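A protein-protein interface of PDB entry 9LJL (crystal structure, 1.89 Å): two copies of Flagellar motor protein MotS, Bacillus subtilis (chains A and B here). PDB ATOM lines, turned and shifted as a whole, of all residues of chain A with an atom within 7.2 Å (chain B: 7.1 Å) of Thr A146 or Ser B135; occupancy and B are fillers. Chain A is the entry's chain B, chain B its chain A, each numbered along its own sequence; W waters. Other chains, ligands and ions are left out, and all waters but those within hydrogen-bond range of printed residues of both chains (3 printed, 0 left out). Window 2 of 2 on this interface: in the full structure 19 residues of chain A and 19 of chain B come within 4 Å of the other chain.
O of Ile B93 lies within hydrogen-bond range of N of Ile B139 (3.1 Å).
The backbone carbonyl oxygen (O) of Ile B124 lies within hydrogen-bond range of the side-chain hydroxyl (OG1) of Thr B128, at 3.0 Å.
OG1 of Thr B128 sits at hydrogen-bond distance from O of Gln B125 (3.4 Å).
The backbone carbonyl oxygen (O) of Gln B125 lies within hydrogen-bond range of the side-chain hydroxyl (OG) of Ser B129.
The backbone carbonyl oxygen (O) of Tyr A143 sits at hydrogen-bond distance from the side-chain hydroxyl (OG1) of Thr A146.
Among the printed residues, merely in contact across the chains: Trp A113 with Ile B124, Trp A113 with Gln B125, Trp A113 with Thr B128, Trp A113 with Ser B135, Trp A113 with Phe B138, Tyr A143 with Ile B139 and Thr A146 with Ser B135.
Of the printed residues of chain B, Trp A113 touches Ile B124, Gln B125, Thr B128, Ser B135 and Phe B138.
Printed residues of chain B within 4 Å of Tyr A143: Ile B139.
Of chain B, only Ser B135 comes within 4 Å of Thr A146.
Of the printed residues of chain A, Thr B128 touches Trp A113 (3.8 Å).
Of chain A, only Trp A113 and Thr A146 come within 4 Å of Ser B135.
Of the printed residues of chain A, Ile B139 touches Tyr A143.
The nearest printed residue of chain A that does not touch Phe B138 is Tyr A143 (4.5 Å).
Of the 13 printed residues of chain B, 6 touch a printed residue of chain A.
Printed residues of chain B that touch a printed residue of chain A: Ile B124, Gln B125, Thr B128, Ser B135, Phe B138 and Ile B139.
Hydrophobic or aromatic side chains of chain B that line the printed part of chain A: Ile B124, Phe B138 and Ile B139.
Among the printed residues, no Asp or Glu carboxylate lies within 4 Å of a Lys or Arg side-chain nitrogen of the other chain.
No position is printed for both chains.
Of the 7 pairs that touch across the chains among the printed residues, none has its exchanged pair printed and touching as well.
Water W2 bridges the side-chain hydroxyl (OG) of Ser B135 (2.5 Å) and the indole nitrogen (NE1) of Trp A113 (3.0 Å).
Water W3 lies within hydrogen-bond range of the backbone carbonyl oxygen (O) of Phe B138 and the side-chain hydroxyl (OG1) of Thr A146.
Water W1 lies within hydrogen-bond range of the side-chain amino group (NZ) of Lys A147 (3.1 Å) and the backbone carbonyl oxygen (O) of Lys B136 (3.2 Å).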
ATOM      1  N   HIS A  98     -29.505  21.041  -0.017  1.00  0.00           N
ATOM      2  CA  HIS A  98     -29.864  20.737  -1.396  1.00  0.00           C
ATOM      3  C   HIS A  98     -31.379  20.701  -1.521  1.00  0.00           C
ATOM      4  O   HIS A  98     -32.057  20.119  -0.673  1.00  0.00           O
ATOM      5  CB  HIS A  98     -29.312  19.365  -1.842  1.00  0.00           C
ATOM      6  CG  HIS A  98     -27.816  19.268  -1.837  1.00  0.00           C
ATOM      7  ND1 HIS A  98     -27.044  19.539  -2.945  1.00  0.00           N
ATOM      8  CD2 HIS A  98     -26.955  18.898  -0.861  1.00  0.00           C
ATOM      9  CE1 HIS A  98     -25.771  19.353  -2.649  1.00  0.00           C
ATOM     10  NE2 HIS A  98     -25.689  18.955  -1.391  1.00  0.00           N
ATOM     11  N   THR A  99     -31.908  21.297  -2.587  1.00  0.00           N
ATOM     12  CA  THR A  99     -33.334  21.254  -2.886  1.00  0.00           C
ATOM     13  C   THR A  99     -33.583  20.395  -4.118  1.00  0.00           C
ATOM     14  O   THR A  99     -32.653  19.936  -4.786  1.00  0.00           O
ATOM     15  CB  THR A  99     -33.895  22.661  -3.137  1.00  0.00           C
ATOM     16  OG1 THR A  99     -33.312  23.196  -4.334  1.00  0.00           O
ATOM     17  CG2 THR A  99     -33.566  23.579  -1.971  1.00  0.00           C
ATOM     18  N   ASP A 100     -34.863  20.188  -4.432  1.00  0.00           N
ATOM     19  CA  ASP A 100     -35.203  19.701  -5.760  1.00  0.00           C
ATOM     20  C   ASP A 100     -35.435  20.919  -6.654  1.00  0.00           C
ATOM     21  O   ASP A 100     -35.222  22.065  -6.243  1.00  0.00           O
ATOM     22  CB  ASP A 100     -36.402  18.743  -5.731  1.00  0.00           C
ATOM     23  CG  ASP A 100     -37.669  19.369  -5.161  1.00  0.00           C
ATOM     24  OD1 ASP A 100     -37.805  20.610  -5.158  1.00  0.00           O
ATOM     25  OD2 ASP A 100     -38.561  18.596  -4.747  1.00  0.00           O
ATOM     26  N   TRP A 113     -31.818  28.821  -3.710  1.00  0.00           N
ATOM     27  CA  TRP A 113     -30.521  29.152  -3.131  1.00  0.00           C
ATOM     28  C   TRP A 113     -30.669  29.504  -1.661  1.00  0.00           C
ATOM     29  O   TRP A 113     -29.979  28.943  -0.804  1.00  0.00           O
ATOM     30  CB  TRP A 113     -29.861  30.302  -3.895  1.00  0.00           C
ATOM     31  CG  TRP A 113     -29.323  29.881  -5.205  1.00  0.00           C
ATOM     32  CD1 TRP A 113     -29.855  30.143  -6.433  1.00  0.00           C
ATOM     33  CD2 TRP A 113     -28.156  29.080  -5.433  1.00  0.00           C
ATOM     34  NE1 TRP A 113     -29.075  29.582  -7.415  1.00  0.00           N
ATOM     35  CE2 TRP A 113     -28.029  28.918  -6.827  1.00  0.00           C
ATOM     36  CE3 TRP A 113     -27.196  28.504  -4.595  1.00  0.00           C
ATOM     37  CZ2 TRP A 113     -26.993  28.193  -7.401  1.00  0.00           C
ATOM     38  CZ3 TRP A 113     -26.163  27.783  -5.166  1.00  0.00           C
ATOM     39  CH2 TRP A 113     -26.068  27.636  -6.559  1.00  0.00           C
ATOM     40  N   GLY A 142     -24.865  26.174   0.503  1.00  0.00           N
ATOM     41  CA  GLY A 142     -26.101  25.950  -0.226  1.00  0.00           C
ATOM     42  C   GLY A 142     -25.862  25.672  -1.698  1.00  0.00           C
ATOM     43  O   GLY A 142     -25.130  26.419  -2.363  1.00  0.00           O
ATOM     44  N   TYR A 143     -26.472  24.603  -2.221  1.00  0.00           N
ATOM     45  CA  TYR A 143     -26.321  24.210  -3.615  1.00  0.00           C
ATOM     46  C   TYR A 143     -27.596  24.339  -4.432  1.00  0.00           C
ATOM     47  O   TYR A 143     -27.576  24.014  -5.624  1.00  0.00           O
ATOM     48  CB  TYR A 143     -25.820  22.760  -3.717  1.00  0.00           C
ATOM     49  CG  TYR A 143     -24.320  22.610  -3.631  1.00  0.00           C
ATOM     50  CD1 TYR A 143     -23.512  22.976  -4.700  1.00  0.00           C
ATOM     51  CD2 TYR A 143     -23.713  22.083  -2.497  1.00  0.00           C
ATOM     52  CE1 TYR A 143     -22.140  22.836  -4.639  1.00  0.00           C
ATOM     53  CE2 TYR A 143     -22.338  21.930  -2.431  1.00  0.00           C
ATOM     54  CZ  TYR A 143     -21.557  22.312  -3.503  1.00  0.00           C
ATOM     55  OH  TYR A 143     -20.186  22.173  -3.445  1.00  0.00           O
ATOM     56  N   ALA A 144     -28.693  24.790  -3.832  1.00  0.00           N
ATOM     57  CA  ALA A 144     -30.006  24.861  -4.488  1.00  0.00           C
ATOM     58  C   ALA A 144     -30.268  23.496  -5.126  1.00  0.00           C
ATOM     59  O   ALA A 144     -30.080  22.471  -4.456  1.00  0.00           O
ATOM     60  CB  ALA A 144     -30.046  26.052  -5.438  1.00  0.00           C
ATOM     61  N   ASP A 145     -30.670  23.432  -6.395  1.00  0.00           N
ATOM     62  CA  ASP A 145     -30.959  22.170  -7.065  1.00  0.00           C
ATOM     63  C   ASP A 145     -29.862  21.757  -8.037  1.00  0.00           C
ATOM     64  O   ASP A 145     -30.107  20.930  -8.920  1.00  0.00           O
ATOM     65  CB  ASP A 145     -32.303  22.257  -7.791  1.00  0.00           C
ATOM     66  CG  ASP A 145     -32.316  23.319  -8.875  1.00  0.00           C
ATOM     67  OD1 ASP A 145     -31.323  24.068  -9.006  1.00  0.00           O
ATOM     68  OD2 ASP A 145     -33.326  23.406  -9.604  1.00  0.00           O
ATOM     69  N   THR A 146     -28.651  22.309  -7.894  1.00  0.00           N
ATOM     70  CA  THR A 146     -27.600  22.059  -8.874  1.00  0.00           C
ATOM     71  C   THR A 146     -26.985  20.668  -8.768  1.00  0.00           C
ATOM     72  O   THR A 146     -26.295  20.248  -9.700  1.00  0.00           O
ATOM     73  CB  THR A 146     -26.492  23.115  -8.753  1.00  0.00           C
ATOM     74  OG1 THR A 146     -25.862  23.015  -7.464  1.00  0.00           O
ATOM     75  CG2 THR A 146     -27.060  24.522  -8.941  1.00  0.00           C
ATOM     76  N   LYS A 147     -27.224  19.941  -7.680  1.00  0.00           N
ATOM     77  CA  LYS A 147     -26.583  18.649  -7.428  1.00  0.00           C
ATOM     78  C   LYS A 147     -27.639  17.594  -7.110  1.00  0.00           C
ATOM     79  O   LYS A 147     -27.699  17.081  -5.986  1.00  0.00           O
ATOM     80  CB  LYS A 147     -25.586  18.753  -6.273  1.00  0.00           C
ATOM     81  CG  LYS A 147     -24.482  19.781  -6.462  1.00  0.00           C
ATOM     82  CD  LYS A 147     -23.200  19.130  -6.924  1.00  0.00           C
ATOM     83  CE  LYS A 147     -22.126  20.159  -7.203  1.00  0.00           C
ATOM     84  NZ  LYS A 147     -21.324  19.774  -8.393  1.00  0.00           N
ATOM     85  N   PRO A 148     -28.472  17.228  -8.083  1.00  0.00           N
ATOM     86  CA  PRO A 148     -29.454  16.165  -7.838  1.00  0.00           C
ATOM     87  C   PRO A 148     -28.760  14.839  -7.591  1.00  0.00           C
ATOM     88  O   PRO A 148     -27.647  14.597  -8.063  1.00  0.00           O
ATOM     89  CB  PRO A 148     -30.266  16.127  -9.138  1.00  0.00           C
ATOM     90  CG  PRO A 148     -29.282  16.592 -10.175  1.00  0.00           C
ATOM     91  CD  PRO A 148     -28.495  17.675  -9.487  1.00  0.00           C
ATOM     92  N   ASN A 152     -34.547  15.205 -11.623  1.00  0.00           N
ATOM     93  CA  ASN A 152     -35.806  15.700 -11.077  1.00  0.00           C
ATOM     94  C   ASN A 152     -36.992  15.271 -11.942  1.00  0.00           C
ATOM     95  O   ASN A 152     -38.011  15.965 -12.008  1.00  0.00           O
ATOM     96  CB  ASN A 152     -35.770  17.222 -10.921  1.00  0.00           C
ATOM     97  CG  ASN A 152     -34.971  17.677  -9.697  1.00  0.00           C
ATOM     98  OD1 ASN A 152     -35.488  17.699  -8.582  1.00  0.00           O
ATOM     99  ND2 ASN A 152     -33.718  18.042  -9.908  1.00  0.00           N
ATOM    100  N   ARG A 163     -32.410  17.276   0.736  1.00  0.00           N
ATOM    101  CA  ARG A 163     -31.555  16.595   1.693  1.00  0.00           C
ATOM    102  C   ARG A 163     -30.508  17.560   2.216  1.00  0.00           C
ATOM    103  O   ARG A 163     -30.231  18.603   1.617  1.00  0.00           O
ATOM    104  CB  ARG A 163     -30.854  15.400   1.047  1.00  0.00           C
ATOM    105  CG  ARG A 163     -29.743  15.827   0.106  1.00  0.00           C
ATOM    106  CD  ARG A 163     -29.441  14.765  -0.935  1.00  0.00           C
ATOM    107  NE  ARG A 163     -28.219  15.046  -1.682  1.00  0.00           N
ATOM    108  CZ  ARG A 163     -28.161  15.741  -2.810  1.00  0.00           C
ATOM    109  NH1 ARG A 163     -29.238  16.305  -3.333  1.00  0.00           N
ATOM    110  NH2 ARG A 163     -26.995  15.863  -3.438  1.00  0.00           N
ATOM    111  N   ILE B  93     -17.508  29.698  -9.203  1.00  0.00           N
ATOM    112  CA  ILE B  93     -17.609  30.866  -8.330  1.00  0.00           C
ATOM    113  C   ILE B  93     -18.156  30.421  -6.978  1.00  0.00           C
ATOM    114  O   ILE B  93     -19.199  29.763  -6.912  1.00  0.00           O
ATOM    115  CB  ILE B  93     -18.509  31.954  -8.944  1.00  0.00           C
ATOM    116  CG1 ILE B  93     -18.076  32.286 -10.377  1.00  0.00           C
ATOM    117  CG2 ILE B  93     -18.517  33.212  -8.067  1.00  0.00           C
ATOM    118  CD1 ILE B  93     -16.651  32.786 -10.505  1.00  0.00           C
ATOM    119  N   ILE B 124     -26.068  35.204  -5.391  1.00  0.00           N
ATOM    120  CA  ILE B 124     -26.083  34.166  -6.420  1.00  0.00           C
ATOM    121  C   ILE B 124     -27.424  34.158  -7.142  1.00  0.00           C
ATOM    122  O   ILE B 124     -27.490  33.977  -8.363  1.00  0.00           O
ATOM    123  CB  ILE B 124     -25.768  32.793  -5.795  1.00  0.00           C
ATOM    124  CG1 ILE B 124     -24.290  32.720  -5.427  1.00  0.00           C
ATOM    125  CG2 ILE B 124     -26.121  31.676  -6.762  1.00  0.00           C
ATOM    126  CD1 ILE B 124     -23.930  31.558  -4.546  1.00  0.00           C
ATOM    127  N   GLN B 125     -28.516  34.346  -6.396  1.00  0.00           N
ATOM    128  CA  GLN B 125     -29.833  34.384  -7.022  1.00  0.00           C
ATOM    129  C   GLN B 125     -29.932  35.548  -7.999  1.00  0.00           C
ATOM    130  O   GLN B 125     -30.574  35.424  -9.051  1.00  0.00           O
ATOM    131  CB  GLN B 125     -30.918  34.477  -5.944  1.00  0.00           C
ATOM    132  CG  GLN B 125     -32.339  34.745  -6.441  1.00  0.00           C
ATOM    133  CD  GLN B 125     -32.929  33.605  -7.265  1.00  0.00           C
ATOM    134  OE1 GLN B 125     -32.266  32.600  -7.546  1.00  0.00           O
ATOM    135  NE2 GLN B 125     -34.193  33.757  -7.653  1.00  0.00           N
ATOM    136  N   THR B 128     -27.896  34.433 -11.181  1.00  0.00           N
ATOM    137  CA  THR B 128     -28.515  33.369 -11.963  1.00  0.00           C
ATOM    138  C   THR B 128     -29.877  33.761 -12.526  1.00  0.00           C
ATOM    139  O   THR B 128     -30.164  33.480 -13.695  1.00  0.00           O
ATOM    140  CB  THR B 128     -28.646  32.092 -11.117  1.00  0.00           C
ATOM    141  OG1 THR B 128     -29.460  32.351  -9.966  1.00  0.00           O
ATOM    142  CG2 THR B 128     -27.273  31.603 -10.666  1.00  0.00           C
ATOM    143  N   SER B 129     -30.725  34.414 -11.740  1.00  0.00           N
ATOM    144  CA  SER B 129     -32.071  34.670 -12.231  1.00  0.00           C
ATOM    145  C   SER B 129     -32.181  35.961 -13.039  1.00  0.00           C
ATOM    146  O   SER B 129     -32.968  36.019 -13.987  1.00  0.00           O
ATOM    147  CB  SER B 129     -33.068  34.688 -11.071  1.00  0.00           C
ATOM    148  OG  SER B 129     -33.060  35.943 -10.431  1.00  0.00           O
ATOM    149  N   LYS B 132     -28.599  35.711 -15.660  1.00  0.00           N
ATOM    150  CA  LYS B 132     -28.644  34.485 -16.468  1.00  0.00           C
ATOM    151  C   LYS B 132     -27.304  33.755 -16.510  1.00  0.00           C
ATOM    152  O   LYS B 132     -26.997  33.053 -17.476  1.00  0.00           O
ATOM    153  CB  LYS B 132     -29.151  34.761 -17.889  1.00  0.00           C
ATOM    154  CG  LYS B 132     -30.376  35.680 -17.989  1.00  0.00           C
ATOM    155  CD  LYS B 132     -31.430  35.365 -16.926  1.00  0.00           C
ATOM    156  CE  LYS B 132     -32.796  35.929 -17.304  1.00  0.00           C
ATOM    157  NZ  LYS B 132     -32.883  37.406 -17.108  1.00  0.00           N
ATOM    158  N   LEU B 133     -26.504  33.886 -15.466  1.00  0.00           N
ATOM    159  CA  LEU B 133     -25.317  33.045 -15.386  1.00  0.00           C
ATOM    160  C   LEU B 133     -25.721  31.637 -14.950  1.00  0.00           C
ATOM    161  O   LEU B 133     -26.596  31.487 -14.095  1.00  0.00           O
ATOM    162  CB  LEU B 133     -24.306  33.623 -14.398  1.00  0.00           C
ATOM    163  CG  LEU B 133     -23.348  34.720 -14.887  1.00  0.00           C
ATOM    164  CD1 LEU B 133     -24.070  35.802 -15.673  1.00  0.00           C
ATOM    165  CD2 LEU B 133     -22.596  35.320 -13.715  1.00  0.00           C
ATOM    166  N   PRO B 134     -25.107  30.595 -15.514  1.00  0.00           N
ATOM    167  CA  PRO B 134     -25.528  29.221 -15.189  1.00  0.00           C
ATOM    168  C   PRO B 134     -25.411  28.914 -13.702  1.00  0.00           C
ATOM    169  O   PRO B 134     -24.372  29.148 -13.080  1.00  0.00           O
ATOM    170  CB  PRO B 134     -24.577  28.351 -16.020  1.00  0.00           C
ATOM    171  CG  PRO B 134     -24.044  29.269 -17.088  1.00  0.00           C
ATOM    172  CD  PRO B 134     -23.967  30.615 -16.446  1.00  0.00           C
ATOM    173  N   SER B 135     -26.497  28.371 -13.140  1.00  0.00           N
ATOM    174  CA  SER B 135     -26.529  28.024 -11.719  1.00  0.00           C
ATOM    175  C   SER B 135     -25.399  27.075 -11.344  1.00  0.00           C
ATOM    176  O   SER B 135     -24.830  27.181 -10.251  1.00  0.00           O
ATOM    177  CB  SER B 135     -27.875  27.390 -11.359  1.00  0.00           C
ATOM    178  OG  SER B 135     -28.953  28.259 -11.648  1.00  0.00           O
ATOM    179  N   LYS B 136     -25.046  26.154 -12.243  1.00  0.00           N
ATOM    180  CA  LYS B 136     -24.032  25.152 -11.939  1.00  0.00           C
ATOM    181  C   LYS B 136     -22.659  25.755 -11.659  1.00  0.00           C
ATOM    182  O   LYS B 136     -21.765  25.044 -11.191  1.00  0.00           O
ATOM    183  CB  LYS B 136     -23.972  24.131 -13.082  1.00  0.00           C
ATOM    184  CG  LYS B 136     -23.369  24.613 -14.414  1.00  0.00           C
ATOM    185  CD  LYS B 136     -21.875  24.296 -14.554  1.00  0.00           C
ATOM    186  CE  LYS B 136     -21.179  25.317 -15.462  1.00  0.00           C
ATOM    187  NZ  LYS B 136     -19.691  25.184 -15.521  1.00  0.00           N
ATOM    188  N   ARG B 137     -22.471  27.050 -11.905  1.00  0.00           N
ATOM    189  CA  ARG B 137     -21.186  27.673 -11.614  1.00  0.00           C
ATOM    190  C   ARG B 137     -21.028  28.090 -10.157  1.00  0.00           C
ATOM    191  O   ARG B 137     -19.907  28.424  -9.748  1.00  0.00           O
ATOM    192  CB  ARG B 137     -20.981  28.896 -12.507  1.00  0.00           C
ATOM    193  CG  ARG B 137     -20.727  28.546 -13.957  1.00  0.00           C
ATOM    194  CD  ARG B 137     -20.307  29.784 -14.724  1.00  0.00           C
ATOM    195  NE  ARG B 137     -19.079  30.395 -14.228  1.00  0.00           N
ATOM    196  CZ  ARG B 137     -18.599  31.537 -14.702  1.00  0.00           C
ATOM    197  NH1 ARG B 137     -19.232  32.204 -15.652  1.00  0.00           N
ATOM    198  NH2 ARG B 137     -17.463  32.025 -14.212  1.00  0.00           N
ATOM    199  N   PHE B 138     -22.091  28.067  -9.363  1.00  0.00           N
ATOM    200  CA  PHE B 138     -22.097  28.770  -8.089  1.00  0.00           C
ATOM    201  C   PHE B 138     -22.262  27.834  -6.901  1.00  0.00           C
ATOM    202  O   PHE B 138     -22.908  26.785  -6.982  1.00  0.00           O
ATOM    203  CB  PHE B 138     -23.208  29.818  -8.056  1.00  0.00           C
ATOM    204  CG  PHE B 138     -23.016  30.934  -9.044  1.00  0.00           C
ATOM    205  CD1 PHE B 138     -22.133  31.971  -8.774  1.00  0.00           C
ATOM    206  CD2 PHE B 138     -23.703  30.939 -10.245  1.00  0.00           C
ATOM    207  CE1 PHE B 138     -21.949  33.007  -9.689  1.00  0.00           C
ATOM    208  CE2 PHE B 138     -23.525  31.966 -11.166  1.00  0.00           C
ATOM    209  CZ  PHE B 138     -22.644  32.995 -10.887  1.00  0.00           C
ATOM    210  N   ILE B 139     -21.678  28.252  -5.783  1.00  0.00           N
ATOM    211  CA  ILE B 139     -21.899  27.647  -4.477  1.00  0.00           C
ATOM    212  C   ILE B 139     -22.060  28.788  -3.480  1.00  0.00           C
ATOM    213  O   ILE B 139     -21.285  29.750  -3.507  1.00  0.00           O
ATOM    214  CB  ILE B 139     -20.732  26.716  -4.086  1.00  0.00           C
ATOM    215  CG1 ILE B 139     -20.749  26.392  -2.598  1.00  0.00           C
ATOM    216  CG2 ILE B 139     -19.406  27.331  -4.451  1.00  0.00           C
ATOM    217  CD1 ILE B 139     -19.684  25.397  -2.221  1.00  0.00           C
HETATM  218  O   HOH W   1     -22.472  22.373  -9.558  1.00  0.00           O
HETATM  219  O   HOH W   2     -30.631  28.906  -9.945  1.00  0.00           O
HETATM  220  O   HOH W   3     -22.899  24.157  -7.815  1.00  0.00           O
